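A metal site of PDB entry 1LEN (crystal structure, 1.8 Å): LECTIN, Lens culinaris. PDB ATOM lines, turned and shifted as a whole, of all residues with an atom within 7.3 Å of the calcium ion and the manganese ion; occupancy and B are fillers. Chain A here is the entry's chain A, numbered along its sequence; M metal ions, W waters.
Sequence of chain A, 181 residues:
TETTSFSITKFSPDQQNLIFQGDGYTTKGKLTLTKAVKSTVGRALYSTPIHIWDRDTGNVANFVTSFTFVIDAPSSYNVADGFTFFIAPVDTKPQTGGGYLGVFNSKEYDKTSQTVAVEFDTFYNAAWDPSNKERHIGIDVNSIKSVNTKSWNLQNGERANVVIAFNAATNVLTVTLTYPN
The side-chain carboxylate (OE1) of Glu 119 sits close to the side-chain carboxylate (OD2) of Asp 140 (2.6 Å).
OG of Ser 146 sits close to OE2 of Glu 119.
A ring nitrogen (ND1) of His 136 lies within hydrogen-bond range of the backbone carbonyl oxygen (O) of Glu 134 (3.0 Å).
The backbone carbonyl oxygen (O) of Glu 119 lies within hydrogen-bond range of the backbone NH (N) of Gly 138.
Four residues have an atom within 4 Å of the calcium ion: Asp 121, Phe 123, Asn 125 and Asp 129.
Four residues have an atom within 4 Å of the manganese ion: Glu 119, Asp 121, Asp 129 and His 136.
The nearest printed residue that does not touch the manganese ion is Ser 146 (4.2 Å).
The calcium ion is bound by OD1 of Asn 125, O of Phe 123, OD2 of Asp 121, water W4, OD2 of Asp 129, water W2 and OD1 of Asp 121.
The calcium ion has seven donor atoms within binding distance.
The manganese ion is bound by water W1 (2.1 Å), water W3 (2.2 Å), a ring nitrogen (NE2) of His 136 (2.2 Å), the side-chain carboxylate of Asp 129 (2.3 Å), the side-chain carboxylate of Asp 121 (2.4 Å) and the side-chain carboxylate of Glu 119 (2.4 Å).
Water W4 lies within hydrogen-bond range of O of Gly 99 (2.9 Å) and NE1 of Trp 128 (3.1 Å).
Water W3 bridges OE1 of Glu 119 (2.7 Å) and O of Ile 144 (2.9 Å).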
ATOM      1  N   ASP A  81     -25.324  12.487   1.015  1.00  0.00           N
ATOM      2  CA  ASP A  81     -25.498  12.955  -0.356  1.00  0.00           C
ATOM      3  C   ASP A  81     -26.292  11.909  -1.150  1.00  0.00           C
ATOM      4  O   ASP A  81     -26.978  12.187  -2.099  1.00  0.00           O
ATOM      5  CB  ASP A  81     -24.135  13.108  -1.073  1.00  0.00           C
ATOM      6  CG  ASP A  81     -23.731  14.607  -1.061  1.00  0.00           C
ATOM      7  OD1 ASP A  81     -24.372  15.373  -1.749  1.00  0.00           O
ATOM      8  OD2 ASP A  81     -22.822  14.946  -0.290  1.00  0.00           O
ATOM      9  N   GLY A  82     -26.120  10.683  -0.617  1.00  0.00           N
ATOM     10  CA  GLY A  82     -26.843   9.609  -1.335  1.00  0.00           C
ATOM     11  C   GLY A  82     -26.083   8.295  -1.371  1.00  0.00           C
ATOM     12  O   GLY A  82     -24.981   8.150  -0.898  1.00  0.00           O
ATOM     13  N   GLY A  98     -18.832  13.717  -2.137  1.00  0.00           N
ATOM     14  CA  GLY A  98     -19.975  14.590  -1.984  1.00  0.00           C
ATOM     15  C   GLY A  98     -21.014  14.309  -3.031  1.00  0.00           C
ATOM     16  O   GLY A  98     -21.349  13.154  -3.156  1.00  0.00           O
ATOM     17  N   GLY A  99     -21.548  15.255  -3.737  1.00  0.00           N
ATOM     18  CA  GLY A  99     -22.578  15.142  -4.753  1.00  0.00           C
ATOM     19  C   GLY A  99     -22.186  14.192  -5.890  1.00  0.00           C
ATOM     20  O   GLY A  99     -23.097  13.779  -6.586  1.00  0.00           O
ATOM     21  N   TYR A 100     -20.943  13.826  -6.096  1.00  0.00           N
ATOM     22  CA  TYR A 100     -20.538  12.921  -7.170  1.00  0.00           C
ATOM     23  C   TYR A 100     -20.677  11.478  -6.786  1.00  0.00           C
ATOM     24  O   TYR A 100     -20.481  10.620  -7.625  1.00  0.00           O
ATOM     25  CB  TYR A 100     -19.196  13.225  -7.729  1.00  0.00           C
ATOM     26  CG  TYR A 100     -19.148  14.560  -8.510  1.00  0.00           C
ATOM     27  CD1 TYR A 100     -19.438  14.667  -9.845  1.00  0.00           C
ATOM     28  CD2 TYR A 100     -18.712  15.644  -7.773  1.00  0.00           C
ATOM     29  CE1 TYR A 100     -19.317  15.950 -10.411  1.00  0.00           C
ATOM     30  CE2 TYR A 100     -18.581  16.897  -8.326  1.00  0.00           C
ATOM     31  CZ  TYR A 100     -18.886  17.023  -9.667  1.00  0.00           C
ATOM     32  OH  TYR A 100     -18.747  18.283 -10.167  1.00  0.00           O
ATOM     33  N   LEU A 101     -21.022  11.227  -5.544  1.00  0.00           N
ATOM     34  CA  LEU A 101     -21.318   9.940  -4.970  1.00  0.00           C
ATOM     35  C   LEU A 101     -20.162   8.985  -4.947  1.00  0.00           C
ATOM     36  O   LEU A 101     -20.453   7.794  -4.772  1.00  0.00           O
ATOM     37  CB  LEU A 101     -22.554   9.287  -5.604  1.00  0.00           C
ATOM     38  CG  LEU A 101     -23.803  10.139  -5.448  1.00  0.00           C
ATOM     39  CD1 LEU A 101     -25.019   9.727  -6.280  1.00  0.00           C
ATOM     40  CD2 LEU A 101     -24.204  10.359  -4.012  1.00  0.00           C
ATOM     41  N   GLU A 119     -28.610   5.655  -8.745  1.00  0.00           N
ATOM     42  CA  GLU A 119     -28.489   6.465  -7.553  1.00  0.00           C
ATOM     43  C   GLU A 119     -29.795   6.680  -6.840  1.00  0.00           C
ATOM     44  O   GLU A 119     -30.887   6.660  -7.393  1.00  0.00           O
ATOM     45  CB  GLU A 119     -27.867   7.834  -7.908  1.00  0.00           C
ATOM     46  CG  GLU A 119     -28.827   8.500  -8.892  1.00  0.00           C
ATOM     47  CD  GLU A 119     -28.490   9.936  -9.101  1.00  0.00           C
ATOM     48  OE1 GLU A 119     -27.359  10.306  -9.410  1.00  0.00           O
ATOM     49  OE2 GLU A 119     -29.329  10.834  -8.959  1.00  0.00           O
ATOM     50  N   PHE A 120     -29.671   6.864  -5.571  1.00  0.00           N
ATOM     51  CA  PHE A 120     -30.658   7.165  -4.504  1.00  0.00           C
ATOM     52  C   PHE A 120     -30.092   8.417  -3.818  1.00  0.00           C
ATOM     53  O   PHE A 120     -29.328   8.467  -2.933  1.00  0.00           O
ATOM     54  CB  PHE A 120     -30.749   5.977  -3.555  1.00  0.00           C
ATOM     55  CG  PHE A 120     -31.144   4.707  -4.294  1.00  0.00           C
ATOM     56  CD1 PHE A 120     -32.490   4.424  -4.502  1.00  0.00           C
ATOM     57  CD2 PHE A 120     -30.149   3.834  -4.778  1.00  0.00           C
ATOM     58  CE1 PHE A 120     -32.855   3.266  -5.204  1.00  0.00           C
ATOM     59  CE2 PHE A 120     -30.515   2.675  -5.470  1.00  0.00           C
ATOM     60  CZ  PHE A 120     -31.870   2.396  -5.677  1.00  0.00           C
ATOM     61  N   ASP A 121     -30.414   9.501  -4.509  1.00  0.00           N
ATOM     62  CA  ASP A 121     -29.958  10.866  -4.271  1.00  0.00           C
ATOM     63  C   ASP A 121     -30.878  11.643  -3.347  1.00  0.00           C
ATOM     64  O   ASP A 121     -32.017  11.959  -3.583  1.00  0.00           O
ATOM     65  CB  ASP A 121     -29.820  11.604  -5.615  1.00  0.00           C
ATOM     66  CG  ASP A 121     -29.003  12.878  -5.527  1.00  0.00           C
ATOM     67  OD1 ASP A 121     -28.685  13.406  -4.452  1.00  0.00           O
ATOM     68  OD2 ASP A 121     -28.533  13.456  -6.545  1.00  0.00           O
ATOM     69  N   THR A 122     -30.292  11.962  -2.184  1.00  0.00           N
ATOM     70  CA  THR A 122     -30.972  12.627  -1.098  1.00  0.00           C
ATOM     71  C   THR A 122     -30.689  14.107  -1.019  1.00  0.00           C
ATOM     72  O   THR A 122     -31.334  14.719  -0.151  1.00  0.00           O
ATOM     73  CB  THR A 122     -30.616  11.953   0.236  1.00  0.00           C
ATOM     74  OG1 THR A 122     -29.215  12.024   0.476  1.00  0.00           O
ATOM     75  CG2 THR A 122     -31.032  10.511   0.196  1.00  0.00           C
ATOM     76  N   PHE A 123     -29.832  14.698  -1.783  1.00  0.00           N
ATOM     77  CA  PHE A 123     -29.443  16.118  -1.696  1.00  0.00           C
ATOM     78  C   PHE A 123     -29.345  16.766  -3.062  1.00  0.00           C
ATOM     79  O   PHE A 123     -28.640  16.333  -3.990  1.00  0.00           O
ATOM     80  CB  PHE A 123     -28.127  16.220  -0.967  1.00  0.00           C
ATOM     81  CG  PHE A 123     -27.629  17.635  -0.736  1.00  0.00           C
ATOM     82  CD1 PHE A 123     -28.047  18.286   0.431  1.00  0.00           C
ATOM     83  CD2 PHE A 123     -26.759  18.209  -1.638  1.00  0.00           C
ATOM     84  CE1 PHE A 123     -27.526  19.564   0.588  1.00  0.00           C
ATOM     85  CE2 PHE A 123     -26.254  19.498  -1.457  1.00  0.00           C
ATOM     86  CZ  PHE A 123     -26.670  20.156  -0.319  1.00  0.00           C
ATOM     87  N   TYR A 124     -30.071  17.859  -3.191  1.00  0.00           N
ATOM     88  CA  TYR A 124     -30.194  18.649  -4.413  1.00  0.00           C
ATOM     89  C   TYR A 124     -28.939  19.400  -4.763  1.00  0.00           C
ATOM     90  O   TYR A 124     -28.618  20.378  -4.073  1.00  0.00           O
ATOM     91  CB  TYR A 124     -31.352  19.639  -4.253  1.00  0.00           C
ATOM     92  CG  TYR A 124     -31.461  20.582  -5.438  1.00  0.00           C
ATOM     93  CD1 TYR A 124     -31.898  20.085  -6.651  1.00  0.00           C
ATOM     94  CD2 TYR A 124     -31.129  21.933  -5.286  1.00  0.00           C
ATOM     95  CE1 TYR A 124     -31.990  20.964  -7.697  1.00  0.00           C
ATOM     96  CE2 TYR A 124     -31.210  22.788  -6.348  1.00  0.00           C
ATOM     97  CZ  TYR A 124     -31.642  22.303  -7.569  1.00  0.00           C
ATOM     98  OH  TYR A 124     -31.770  23.132  -8.668  1.00  0.00           O
ATOM     99  N   ASN A 125     -28.194  19.004  -5.784  1.00  0.00           N
ATOM    100  CA  ASN A 125     -26.995  19.773  -6.243  1.00  0.00           C
ATOM    101  C   ASN A 125     -27.498  20.610  -7.428  1.00  0.00           C
ATOM    102  O   ASN A 125     -27.941  20.049  -8.410  1.00  0.00           O
ATOM    103  CB  ASN A 125     -25.929  18.813  -6.726  1.00  0.00           C
ATOM    104  CG  ASN A 125     -25.489  17.955  -5.527  1.00  0.00           C
ATOM    105  OD1 ASN A 125     -26.113  16.835  -5.268  1.00  0.00           O
ATOM    106  ND2 ASN A 125     -24.508  18.481  -4.824  1.00  0.00           N
ATOM    107  N   ALA A 126     -27.556  21.888  -7.278  1.00  0.00           N
ATOM    108  CA  ALA A 126     -28.106  22.781  -8.285  1.00  0.00           C
ATOM    109  C   ALA A 126     -27.478  22.642  -9.637  1.00  0.00           C
ATOM    110  O   ALA A 126     -28.221  22.845 -10.636  1.00  0.00           O
ATOM    111  CB  ALA A 126     -28.090  24.213  -7.799  1.00  0.00           C
ATOM    112  N   TRP A 128     -26.729  20.065 -11.414  1.00  0.00           N
ATOM    113  CA  TRP A 128     -27.220  19.019 -12.348  1.00  0.00           C
ATOM    114  C   TRP A 128     -28.423  18.302 -11.814  1.00  0.00           C
ATOM    115  O   TRP A 128     -28.912  17.522 -12.644  1.00  0.00           O
ATOM    116  CB  TRP A 128     -26.081  17.994 -12.558  1.00  0.00           C
ATOM    117  CG  TRP A 128     -25.634  17.379 -11.218  1.00  0.00           C
ATOM    118  CD1 TRP A 128     -26.297  16.437 -10.516  1.00  0.00           C
ATOM    119  CD2 TRP A 128     -24.454  17.684 -10.524  1.00  0.00           C
ATOM    120  NE1 TRP A 128     -25.523  16.168  -9.347  1.00  0.00           N
ATOM    121  CE2 TRP A 128     -24.443  16.929  -9.378  1.00  0.00           C
ATOM    122  CE3 TRP A 128     -23.383  18.565 -10.753  1.00  0.00           C
ATOM    123  CZ2 TRP A 128     -23.429  17.001  -8.485  1.00  0.00           C
ATOM    124  CZ3 TRP A 128     -22.384  18.626  -9.832  1.00  0.00           C
ATOM    125  CH2 TRP A 128     -22.371  17.847  -8.681  1.00  0.00           C
ATOM    126  N   ASP A 129     -28.941  18.372 -10.611  1.00  0.00           N
ATOM    127  CA  ASP A 129     -30.109  17.555 -10.193  1.00  0.00           C
ATOM    128  C   ASP A 129     -31.399  18.143 -10.717  1.00  0.00           C
ATOM    129  O   ASP A 129     -31.360  19.331 -11.019  1.00  0.00           O
ATOM    130  CB  ASP A 129     -30.172  17.519  -8.640  1.00  0.00           C
ATOM    131  CG  ASP A 129     -29.192  16.504  -8.099  1.00  0.00           C
ATOM    132  OD1 ASP A 129     -29.023  15.506  -8.818  1.00  0.00           O
ATOM    133  OD2 ASP A 129     -28.580  16.544  -7.033  1.00  0.00           O
ATOM    134  N   PRO A 130     -32.476  17.357 -10.774  1.00  0.00           N
ATOM    135  CA  PRO A 130     -33.768  17.876 -11.242  1.00  0.00           C
ATOM    136  C   PRO A 130     -34.153  19.133 -10.505  1.00  0.00           C
ATOM    137  O   PRO A 130     -34.006  19.254  -9.292  1.00  0.00           O
ATOM    138  CB  PRO A 130     -34.683  16.729 -10.941  1.00  0.00           C
ATOM    139  CG  PRO A 130     -33.888  15.472 -10.727  1.00  0.00           C
ATOM    140  CD  PRO A 130     -32.490  15.936 -10.434  1.00  0.00           C
ATOM    141  N   GLU A 134     -36.484  17.772  -5.604  1.00  0.00           N
ATOM    142  CA  GLU A 134     -36.960  16.590  -4.854  1.00  0.00           C
ATOM    143  C   GLU A 134     -35.885  15.533  -4.774  1.00  0.00           C
ATOM    144  O   GLU A 134     -35.011  15.407  -5.615  1.00  0.00           O
ATOM    145  CB  GLU A 134     -38.176  16.028  -5.579  1.00  0.00           C
ATOM    146  CG  GLU A 134     -39.381  16.132  -4.685  1.00  0.00           C
ATOM    147  CD  GLU A 134     -40.649  16.414  -5.466  1.00  0.00           C
ATOM    148  OE1 GLU A 134     -40.902  17.601  -5.741  1.00  0.00           O
ATOM    149  OE2 GLU A 134     -41.436  15.522  -5.801  1.00  0.00           O
ATOM    150  N   HIS A 136     -34.471  11.788  -5.269  1.00  0.00           N
ATOM    151  CA  HIS A 136     -34.983  10.991  -6.401  1.00  0.00           C
ATOM    152  C   HIS A 136     -34.096   9.767  -6.671  1.00  0.00           C
ATOM    153  O   HIS A 136     -32.958   9.643  -6.255  1.00  0.00           O
ATOM    154  CB  HIS A 136     -34.820  11.901  -7.672  1.00  0.00           C
ATOM    155  CG  HIS A 136     -33.485  12.631  -7.759  1.00  0.00           C
ATOM    156  ND1 HIS A 136     -33.046  13.731  -7.050  1.00  0.00           N
ATOM    157  CD2 HIS A 136     -32.390  12.297  -8.566  1.00  0.00           C
ATOM    158  CE1 HIS A 136     -31.774  14.076  -7.373  1.00  0.00           C
ATOM    159  NE2 HIS A 136     -31.337  13.196  -8.328  1.00  0.00           N
ATOM    160  N   ILE A 137     -34.697   8.863  -7.429  1.00  0.00           N
ATOM    161  CA  ILE A 137     -33.926   7.692  -7.894  1.00  0.00           C
ATOM    162  C   ILE A 137     -33.410   8.020  -9.300  1.00  0.00           C
ATOM    163  O   ILE A 137     -34.171   8.623 -10.070  1.00  0.00           O
ATOM    164  CB  ILE A 137     -34.822   6.464  -7.982  1.00  0.00           C
ATOM    165  CG1 ILE A 137     -35.422   6.147  -6.605  1.00  0.00           C
ATOM    166  CG2 ILE A 137     -34.012   5.263  -8.484  1.00  0.00           C
ATOM    167  CD1 ILE A 137     -36.744   5.405  -6.809  1.00  0.00           C
ATOM    168  N   GLY A 138     -32.220   7.732  -9.734  1.00  0.00           N
ATOM    169  CA  GLY A 138     -31.852   8.113 -11.089  1.00  0.00           C
ATOM    170  C   GLY A 138     -30.983   7.059 -11.751  1.00  0.00           C
ATOM    171  O   GLY A 138     -30.378   6.234 -11.076  1.00  0.00           O
ATOM    172  N   ASP A 140     -27.710   6.693 -14.131  1.00  0.00           N
ATOM    173  CA  ASP A 140     -26.540   7.453 -14.501  1.00  0.00           C
ATOM    174  C   ASP A 140     -25.617   6.683 -15.413  1.00  0.00           C
ATOM    175  O   ASP A 140     -25.239   5.609 -15.007  1.00  0.00           O
ATOM    176  CB  ASP A 140     -25.738   7.881 -13.258  1.00  0.00           C
ATOM    177  CG  ASP A 140     -26.500   8.673 -12.225  1.00  0.00           C
ATOM    178  OD1 ASP A 140     -27.637   9.083 -12.388  1.00  0.00           O
ATOM    179  OD2 ASP A 140     -25.934   8.912 -11.154  1.00  0.00           O
ATOM    180  N   ILE A 144     -22.755  12.237 -13.611  1.00  0.00           N
ATOM    181  CA  ILE A 144     -23.550  12.450 -12.398  1.00  0.00           C
ATOM    182  C   ILE A 144     -24.930  12.963 -12.725  1.00  0.00           C
ATOM    183  O   ILE A 144     -25.896  12.924 -12.006  1.00  0.00           O
ATOM    184  CB  ILE A 144     -22.845  13.316 -11.392  1.00  0.00           C
ATOM    185  CG1 ILE A 144     -23.373  13.138  -9.981  1.00  0.00           C
ATOM    186  CG2 ILE A 144     -22.787  14.777 -11.793  1.00  0.00           C
ATOM    187  CD1 ILE A 144     -23.447  11.735  -9.422  1.00  0.00           C
ATOM    188  N   LYS A 145     -25.044  13.488 -13.938  1.00  0.00           N
ATOM    189  CA  LYS A 145     -26.328  14.039 -14.460  1.00  0.00           C
ATOM    190  C   LYS A 145     -27.200  12.869 -14.924  1.00  0.00           C
ATOM    191  O   LYS A 145     -26.911  12.418 -16.036  1.00  0.00           O
ATOM    192  CB  LYS A 145     -25.926  14.844 -15.733  1.00  0.00           C
ATOM    193  CG  LYS A 145     -26.530  16.194 -15.573  1.00  0.00           C
ATOM    194  CD  LYS A 145     -27.903  16.111 -16.185  1.00  0.00           C
ATOM    195  CE  LYS A 145     -27.769  16.773 -17.578  1.00  0.00           C
ATOM    196  NZ  LYS A 145     -28.704  16.057 -18.460  1.00  0.00           N
ATOM    197  N   SER A 146     -28.168  12.327 -14.295  1.00  0.00           N
ATOM    198  CA  SER A 146     -28.938  11.155 -14.707  1.00  0.00           C
ATOM    199  C   SER A 146     -29.596  11.269 -16.045  1.00  0.00           C
ATOM    200  O   SER A 146     -30.173  12.279 -16.428  1.00  0.00           O
ATOM    201  CB  SER A 146     -30.010  10.846 -13.653  1.00  0.00           C
ATOM    202  OG  SER A 146     -29.453  10.968 -12.362  1.00  0.00           O
ATOM    203  N   THR A 149     -34.777  10.119 -14.091  1.00  0.00           N
ATOM    204  CA  THR A 149     -34.958  10.239 -12.645  1.00  0.00           C
ATOM    205  C   THR A 149     -36.439  10.038 -12.300  1.00  0.00           C
ATOM    206  O   THR A 149     -37.311  10.158 -13.136  1.00  0.00           O
ATOM    207  CB  THR A 149     -34.490  11.573 -12.116  1.00  0.00           C
ATOM    208  OG1 THR A 149     -35.310  12.639 -12.561  1.00  0.00           O
ATOM    209  CG2 THR A 149     -33.073  11.875 -12.438  1.00  0.00           C
HETATM  210 CA    CA M   1     -27.466  15.171  -5.496  1.00  0.00          CA
HETATM  211 MN    MN M   2     -29.175  13.207  -8.813  1.00  0.00          MN
HETATM  212  O   HOH W   1     -29.630  13.208 -10.885  1.00  0.00           O
HETATM  213  O   HOH W   2     -26.295  14.260  -3.663  1.00  0.00           O
HETATM  214  O   HOH W   3     -27.081  12.998  -9.371  1.00  0.00           O
HETATM  215  O   HOH W   4     -25.953  14.265  -6.968  1.00  0.00           O
